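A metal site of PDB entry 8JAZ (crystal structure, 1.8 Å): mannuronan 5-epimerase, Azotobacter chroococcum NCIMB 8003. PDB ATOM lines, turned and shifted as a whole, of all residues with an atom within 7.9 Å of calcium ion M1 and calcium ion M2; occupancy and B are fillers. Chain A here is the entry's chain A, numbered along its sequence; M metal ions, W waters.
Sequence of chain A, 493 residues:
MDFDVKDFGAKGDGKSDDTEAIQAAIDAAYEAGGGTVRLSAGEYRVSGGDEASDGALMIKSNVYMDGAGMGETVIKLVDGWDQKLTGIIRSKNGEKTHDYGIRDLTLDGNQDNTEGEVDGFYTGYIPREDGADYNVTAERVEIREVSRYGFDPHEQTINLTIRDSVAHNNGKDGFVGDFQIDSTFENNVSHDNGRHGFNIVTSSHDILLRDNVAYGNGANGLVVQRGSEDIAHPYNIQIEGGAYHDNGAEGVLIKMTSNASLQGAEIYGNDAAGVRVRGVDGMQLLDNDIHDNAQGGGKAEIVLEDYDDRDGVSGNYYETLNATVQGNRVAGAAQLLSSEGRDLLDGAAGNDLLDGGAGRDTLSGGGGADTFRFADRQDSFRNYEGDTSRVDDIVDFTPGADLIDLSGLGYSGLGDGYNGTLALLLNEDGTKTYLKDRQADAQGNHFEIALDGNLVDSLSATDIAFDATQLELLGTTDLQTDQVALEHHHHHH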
ATOM      1  N   VAL A 330      -1.605  16.976  -6.025  1.00  0.00           N
ATOM      2  CA  VAL A 330      -0.234  16.858  -6.506  1.00  0.00           C
ATOM      3  C   VAL A 330      -0.281  16.991  -8.015  1.00  0.00           C
ATOM      4  O   VAL A 330      -0.849  16.144  -8.707  1.00  0.00           O
ATOM      5  CB  VAL A 330       0.411  15.530  -6.087  1.00  0.00           C
ATOM      6  CG1 VAL A 330       1.920  15.592  -6.267  1.00  0.00           C
ATOM      7  CG2 VAL A 330       0.041  15.190  -4.651  1.00  0.00           C
ATOM      8  N   GLY A 332       1.786  16.423 -10.401  1.00  0.00           N
ATOM      9  CA  GLY A 332       2.934  15.737 -10.957  1.00  0.00           C
ATOM     10  C   GLY A 332       3.046  14.331 -10.394  1.00  0.00           C
ATOM     11  O   GLY A 332       2.166  13.852  -9.666  1.00  0.00           O
ATOM     12  N   ALA A 333       4.151  13.675 -10.748  1.00  0.00           N
ATOM     13  CA  ALA A 333       4.353  12.284 -10.369  1.00  0.00           C
ATOM     14  C   ALA A 333       4.665  12.177  -8.876  1.00  0.00           C
ATOM     15  O   ALA A 333       5.455  12.953  -8.331  1.00  0.00           O
ATOM     16  CB  ALA A 333       5.482  11.667 -11.190  1.00  0.00           C
ATOM     17  N   ALA A 334       4.033  11.198  -8.227  1.00  0.00           N
ATOM     18  CA  ALA A 334       4.291  10.891  -6.825  1.00  0.00           C
ATOM     19  C   ALA A 334       4.837   9.468  -6.721  1.00  0.00           C
ATOM     20  O   ALA A 334       4.208   8.518  -7.216  1.00  0.00           O
ATOM     21  CB  ALA A 334       3.016  11.035  -5.988  1.00  0.00           C
ATOM     22  N   ASP A 346      -2.398   7.209  -1.579  1.00  0.00           N
ATOM     23  CA  ASP A 346      -3.283   7.789  -2.574  1.00  0.00           C
ATOM     24  C   ASP A 346      -2.476   8.692  -3.498  1.00  0.00           C
ATOM     25  O   ASP A 346      -1.799   9.615  -3.032  1.00  0.00           O
ATOM     26  CB  ASP A 346      -4.419   8.581  -1.918  1.00  0.00           C
ATOM     27  CG  ASP A 346      -5.383   7.691  -1.151  1.00  0.00           C
ATOM     28  OD1 ASP A 346      -5.271   6.457  -1.277  1.00  0.00           O
ATOM     29  OD2 ASP A 346      -6.246   8.235  -0.429  1.00  0.00           O
ATOM     30  N   GLY A 347      -2.567   8.429  -4.798  1.00  0.00           N
ATOM     31  CA  GLY A 347      -1.964   9.292  -5.794  1.00  0.00           C
ATOM     32  C   GLY A 347      -2.838  10.484  -6.121  1.00  0.00           C
ATOM     33  O   GLY A 347      -3.873  10.736  -5.506  1.00  0.00           O
ATOM     34  N   ALA A 348      -2.399  11.232  -7.129  1.00  0.00           N
ATOM     35  CA  ALA A 348      -3.075  12.455  -7.546  1.00  0.00           C
ATOM     36  C   ALA A 348      -3.030  12.532  -9.072  1.00  0.00           C
ATOM     37  O   ALA A 348      -2.809  11.522  -9.753  1.00  0.00           O
ATOM     38  CB  ALA A 348      -2.460  13.684  -6.866  1.00  0.00           C
ATOM     39  N   ALA A 349      -3.255  13.723  -9.614  1.00  0.00           N
ATOM     40  CA  ALA A 349      -3.439  13.894 -11.055  1.00  0.00           C
ATOM     41  C   ALA A 349      -2.235  13.463 -11.871  1.00  0.00           C
ATOM     42  O   ALA A 349      -2.372  13.232 -13.078  1.00  0.00           O
ATOM     43  CB  ALA A 349      -3.774  15.353 -11.356  1.00  0.00           C
ATOM     44  N   GLY A 350      -1.050  13.351 -11.269  1.00  0.00           N
ATOM     45  CA  GLY A 350       0.132  12.957 -11.994  1.00  0.00           C
ATOM     46  C   GLY A 350       0.193  11.460 -12.251  1.00  0.00           C
ATOM     47  O   GLY A 350      -0.666  10.678 -11.842  1.00  0.00           O
ATOM     48  N   ASN A 351       1.253  11.058 -12.963  1.00  0.00           N
ATOM     49  CA  ASN A 351       1.508   9.647 -13.258  1.00  0.00           C
ATOM     50  C   ASN A 351       2.328   9.073 -12.122  1.00  0.00           C
ATOM     51  O   ASN A 351       3.542   9.248 -12.060  1.00  0.00           O
ATOM     52  CB  ASN A 351       2.226   9.499 -14.598  1.00  0.00           C
ATOM     53  CG  ASN A 351       1.361   9.879 -15.783  1.00  0.00           C
ATOM     54  OD1 ASN A 351       0.148  10.078 -15.637  1.00  0.00           O
ATOM     55  ND2 ASN A 351       1.972   9.987 -16.957  1.00  0.00           N
ATOM     56  N   ASP A 352       1.669   8.354 -11.217  1.00  0.00           N
ATOM     57  CA  ASP A 352       2.258   7.959  -9.950  1.00  0.00           C
ATOM     58  C   ASP A 352       2.683   6.489  -9.962  1.00  0.00           C
ATOM     59  O   ASP A 352       2.178   5.678 -10.742  1.00  0.00           O
ATOM     60  CB  ASP A 352       1.281   8.203  -8.802  1.00  0.00           C
ATOM     61  CG  ASP A 352       0.764   9.620  -8.769  1.00  0.00           C
ATOM     62  OD1 ASP A 352       1.572  10.557  -8.927  1.00  0.00           O
ATOM     63  OD2 ASP A 352      -0.463   9.794  -8.599  1.00  0.00           O
ATOM     64  N   LEU A 353       3.629   6.176  -9.081  1.00  0.00           N
ATOM     65  CA  LEU A 353       4.034   4.808  -8.787  1.00  0.00           C
ATOM     66  C   LEU A 353       3.626   4.491  -7.358  1.00  0.00           C
ATOM     67  O   LEU A 353       3.924   5.255  -6.441  1.00  0.00           O
ATOM     68  CB  LEU A 353       5.554   4.650  -8.959  1.00  0.00           C
ATOM     69  CG  LEU A 353       6.169   3.329  -8.496  1.00  0.00           C
ATOM     70  CD1 LEU A 353       5.622   2.159  -9.299  1.00  0.00           C
ATOM     71  CD2 LEU A 353       7.691   3.390  -8.556  1.00  0.00           C
ATOM     72  N   LEU A 354       2.934   3.365  -7.175  1.00  0.00           N
ATOM     73  CA  LEU A 354       2.475   2.963  -5.853  1.00  0.00           C
ATOM     74  C   LEU A 354       2.927   1.540  -5.565  1.00  0.00           C
ATOM     75  O   LEU A 354       2.742   0.642  -6.386  1.00  0.00           O
ATOM     76  CB  LEU A 354       0.956   3.059  -5.739  1.00  0.00           C
ATOM     77  CG  LEU A 354       0.332   4.442  -5.939  1.00  0.00           C
ATOM     78  CD1 LEU A 354      -0.143   4.619  -7.372  1.00  0.00           C
ATOM     79  CD2 LEU A 354      -0.803   4.657  -4.960  1.00  0.00           C
ATOM     80  N   SER A 364      -4.558   3.843  -4.156  1.00  0.00           N
ATOM     81  CA  SER A 364      -5.388   4.510  -5.144  1.00  0.00           C
ATOM     82  C   SER A 364      -4.510   5.430  -5.971  1.00  0.00           C
ATOM     83  O   SER A 364      -3.646   6.140  -5.435  1.00  0.00           O
ATOM     84  CB  SER A 364      -6.529   5.309  -4.494  1.00  0.00           C
ATOM     85  OG  SER A 364      -6.031   6.438  -3.785  1.00  0.00           O
ATOM     86  N   GLY A 365      -4.733   5.432  -7.283  1.00  0.00           N
ATOM     87  CA  GLY A 365      -3.875   6.179  -8.186  1.00  0.00           C
ATOM     88  C   GLY A 365      -4.346   7.578  -8.501  1.00  0.00           C
ATOM     89  O   GLY A 365      -3.541   8.441  -8.845  1.00  0.00           O
ATOM     90  N   GLY A 366      -5.654   7.819  -8.391  1.00  0.00           N
ATOM     91  CA  GLY A 366      -6.164   9.121  -8.802  1.00  0.00           C
ATOM     92  C   GLY A 366      -6.108   9.285 -10.311  1.00  0.00           C
ATOM     93  O   GLY A 366      -6.168   8.322 -11.083  1.00  0.00           O
ATOM     94  N   GLY A 367      -5.990  10.534 -10.744  1.00  0.00           N
ATOM     95  CA  GLY A 367      -5.897  10.831 -12.150  1.00  0.00           C
ATOM     96  C   GLY A 367      -4.567  10.387 -12.753  1.00  0.00           C
ATOM     97  O   GLY A 367      -3.607  10.046 -12.059  1.00  0.00           O
ATOM     98  N   GLY A 368      -4.527  10.392 -14.087  1.00  0.00           N
ATOM     99  CA  GLY A 368      -3.332  10.007 -14.796  1.00  0.00           C
ATOM    100  C   GLY A 368      -3.183   8.500 -14.912  1.00  0.00           C
ATOM    101  O   GLY A 368      -4.019   7.707 -14.465  1.00  0.00           O
ATOM    102  N   ALA A 369      -2.065   8.097 -15.514  1.00  0.00           N
ATOM    103  CA  ALA A 369      -1.719   6.691 -15.691  1.00  0.00           C
ATOM    104  C   ALA A 369      -0.777   6.290 -14.561  1.00  0.00           C
ATOM    105  O   ALA A 369       0.372   6.727 -14.511  1.00  0.00           O
ATOM    106  CB  ALA A 369      -1.086   6.443 -17.057  1.00  0.00           C
ATOM    107  N   ASP A 370      -1.267   5.436 -13.664  1.00  0.00           N
ATOM    108  CA  ASP A 370      -0.543   5.073 -12.452  1.00  0.00           C
ATOM    109  C   ASP A 370      -0.117   3.619 -12.504  1.00  0.00           C
ATOM    110  O   ASP A 370      -0.863   2.756 -12.974  1.00  0.00           O
ATOM    111  CB  ASP A 370      -1.414   5.312 -11.216  1.00  0.00           C
ATOM    112  CG  ASP A 370      -1.932   6.734 -11.137  1.00  0.00           C
ATOM    113  OD1 ASP A 370      -3.152   6.927 -11.304  1.00  0.00           O
ATOM    114  OD2 ASP A 370      -1.117   7.654 -10.912  1.00  0.00           O
ATOM    115  N   THR A 371       1.087   3.349 -12.022  1.00  0.00           N
ATOM    116  CA  THR A 371       1.613   1.995 -11.910  1.00  0.00           C
ATOM    117  C   THR A 371       1.461   1.507 -10.476  1.00  0.00           C
ATOM    118  O   THR A 371       1.935   2.164  -9.538  1.00  0.00           O
ATOM    119  CB  THR A 371       3.078   1.936 -12.348  1.00  0.00           C
ATOM    120  OG1 THR A 371       3.182   2.256 -13.738  1.00  0.00           O
ATOM    121  CG2 THR A 371       3.641   0.540 -12.112  1.00  0.00           C
ATOM    122  N   PHE A 372       0.805   0.359 -10.303  1.00  0.00           N
ATOM    123  CA  PHE A 372       0.697  -0.297  -9.010  1.00  0.00           C
ATOM    124  C   PHE A 372       1.603  -1.515  -9.047  1.00  0.00           C
ATOM    125  O   PHE A 372       1.287  -2.513  -9.704  1.00  0.00           O
ATOM    126  CB  PHE A 372      -0.753  -0.690  -8.718  1.00  0.00           C
ATOM    127  CG  PHE A 372      -1.724   0.462  -8.767  1.00  0.00           C
ATOM    128  CD1 PHE A 372      -2.043   1.160  -7.615  1.00  0.00           C
ATOM    129  CD2 PHE A 372      -2.321   0.833  -9.958  1.00  0.00           C
ATOM    130  CE1 PHE A 372      -2.941   2.217  -7.650  1.00  0.00           C
ATOM    131  CE2 PHE A 372      -3.215   1.884 -10.005  1.00  0.00           C
ATOM    132  CZ  PHE A 372      -3.521   2.577  -8.854  1.00  0.00           C
ATOM    133  N   ASP A 396      -9.194   2.544  -7.316  1.00  0.00           N
ATOM    134  CA  ASP A 396      -9.714   3.229  -8.501  1.00  0.00           C
ATOM    135  C   ASP A 396      -8.950   2.828  -9.756  1.00  0.00           C
ATOM    136  O   ASP A 396      -8.601   3.670 -10.585  1.00  0.00           O
ATOM    137  CB  ASP A 396      -9.665   4.741  -8.313  1.00  0.00           C
ATOM    138  CG  ASP A 396      -8.254   5.264  -8.164  1.00  0.00           C
ATOM    139  OD1 ASP A 396      -7.371   4.479  -7.735  1.00  0.00           O
ATOM    140  OD2 ASP A 396      -8.016   6.451  -8.477  1.00  0.00           O
ATOM    141  N   PHE A 397      -8.685   1.530  -9.922  1.00  0.00           N
ATOM    142  CA  PHE A 397      -7.945   1.100 -11.105  1.00  0.00           C
ATOM    143  C   PHE A 397      -8.757   1.342 -12.367  1.00  0.00           C
ATOM    144  O   PHE A 397      -9.956   1.018 -12.433  1.00  0.00           O
ATOM    145  CB  PHE A 397      -7.574  -0.382 -11.012  1.00  0.00           C
ATOM    146  CG  PHE A 397      -6.569  -0.798 -12.032  1.00  0.00           C
ATOM    147  CD1 PHE A 397      -6.969  -1.312 -13.249  1.00  0.00           C
ATOM    148  CD2 PHE A 397      -5.209  -0.653 -11.783  1.00  0.00           C
ATOM    149  CE1 PHE A 397      -6.038  -1.678 -14.203  1.00  0.00           C
ATOM    150  CE2 PHE A 397      -4.279  -1.027 -12.725  1.00  0.00           C
ATOM    151  CZ  PHE A 397      -4.687  -1.543 -13.935  1.00  0.00           C
ATOM    152  N   THR A 398      -8.106   1.904 -13.378  1.00  0.00           N
ATOM    153  CA  THR A 398      -8.735   2.236 -14.659  1.00  0.00           C
ATOM    154  C   THR A 398      -8.021   1.454 -15.739  1.00  0.00           C
ATOM    155  O   THR A 398      -6.868   1.775 -16.075  1.00  0.00           O
ATOM    156  CB  THR A 398      -8.681   3.741 -14.954  1.00  0.00           C
ATOM    157  OG1 THR A 398      -7.408   4.083 -15.500  1.00  0.00           O
ATOM    158  CG2 THR A 398      -8.911   4.545 -13.677  1.00  0.00           C
ATOM    159  N   ALA A 401      -5.960   3.247 -18.548  1.00  0.00           N
ATOM    160  CA  ALA A 401      -4.805   4.064 -18.193  1.00  0.00           C
ATOM    161  C   ALA A 401      -3.847   3.384 -17.231  1.00  0.00           C
ATOM    162  O   ALA A 401      -2.634   3.361 -17.473  1.00  0.00           O
ATOM    163  CB  ALA A 401      -5.272   5.400 -17.592  1.00  0.00           C
ATOM    164  N   ASP A 402      -4.351   2.823 -16.132  1.00  0.00           N
ATOM    165  CA  ASP A 402      -3.482   2.325 -15.076  1.00  0.00           C
ATOM    166  C   ASP A 402      -2.864   0.980 -15.450  1.00  0.00           C
ATOM    167  O   ASP A 402      -3.297   0.286 -16.381  1.00  0.00           O
ATOM    168  CB  ASP A 402      -4.254   2.192 -13.769  1.00  0.00           C
ATOM    169  CG  ASP A 402      -4.858   3.508 -13.310  1.00  0.00           C
ATOM    170  OD1 ASP A 402      -4.273   4.569 -13.627  1.00  0.00           O
ATOM    171  OD2 ASP A 402      -5.901   3.468 -12.634  1.00  0.00           O
ATOM    172  N   LEU A 403      -1.817   0.609 -14.697  1.00  0.00           N
ATOM    173  CA  LEU A 403      -1.034  -0.588 -14.959  1.00  0.00           C
ATOM    174  C   LEU A 403      -0.731  -1.287 -13.641  1.00  0.00           C
ATOM    175  O   LEU A 403      -0.389  -0.633 -12.654  1.00  0.00           O
ATOM    176  CB  LEU A 403       0.255  -0.223 -15.710  1.00  0.00           C
ATOM    177  CG  LEU A 403       1.244  -1.230 -16.305  1.00  0.00           C
ATOM    178  CD1 LEU A 403       2.053  -1.976 -15.252  1.00  0.00           C
ATOM    179  CD2 LEU A 403       0.527  -2.204 -17.238  1.00  0.00           C
HETATM  180 CA    CA M   1      -2.264   9.489 -10.365  1.00  0.00          CA
HETATM  181 CA    CA M   2      -5.106   6.638 -12.600  1.00  0.00          CA
HETATM  182  O   HOH W   1      -6.156   5.146 -10.518  1.00  0.00           O
HETATM  183  O   HOH W   2      -6.779   6.869 -14.222  1.00  0.00           O
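The backbone carbonyl oxygen (O) of Asp 370 is in hydrogen-bond range of the backbone NH (N) of Leu 403. The backbone NH of Gly 365 is in hydrogen-bond range of the side-chain carboxylate of Asp 396, at 2.8 Å. The backbone NH (N) of Thr 398 lies within hydrogen-bond range of the side-chain carboxylate (OD2) of Asp 402 (2.8 Å). The backbone NH (N) of Gly 366 lies within hydrogen-bond range of the side-chain carboxylate (OD2) of Asp 396. OD1 of Asp 352 is in hydrogen-bond range of N of Ala 334 (2.6 Å). N of Thr 371 sits at hydrogen-bond distance from O of Asp 352.
Of the 28 residues printed, 7 come within 4 Å of calcium ion M1. The nearest printed residue that does not touch calcium ion M1 is Ala 349 (4.2 Å).
Five residues have an atom within 4 Å of calcium ion M2: Gly 366, Gly 367, Gly 368, Asp 370 and Asp 402.
Calcium ion M1 is bound by the backbone carbonyl oxygen (O) of Ala 348 (2.2 Å), the side-chain carboxylate (OD2) of Asp 370 (2.2 Å), the backbone carbonyl oxygen (O) of Gly 367 (2.2 Å), the backbone carbonyl oxygen (O) of Gly 365 (2.2 Å), the backbone carbonyl oxygen (O) of Gly 350 (2.5 Å), the side-chain carboxylate (OD2) of Asp 352 (2.5 Å) and the side-chain carboxylate (OD1) of Asp 370 (2.9 Å).
Water W2 binds calcium ion M2 (2.3 Å). OD1 of Asp 370 is bound to calcium ion M2. The backbone carbonyl oxygen (O) of Gly 368 binds calcium ion M2 (2.4 Å). OD1 of Asp 402 is bound to calcium ion M2, at 2.5 Å. The backbone carbonyl oxygen (O) of Gly 366 is bound to calcium ion M2, 2.5 Å away. Water W1 binds calcium ion M2 (2.8 Å). Calcium ion M2 has six donor atoms within binding distance.
Water W1 lies within hydrogen-bond range of OD2 of Asp 402, O of Asp 396 and N of Gly 366.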
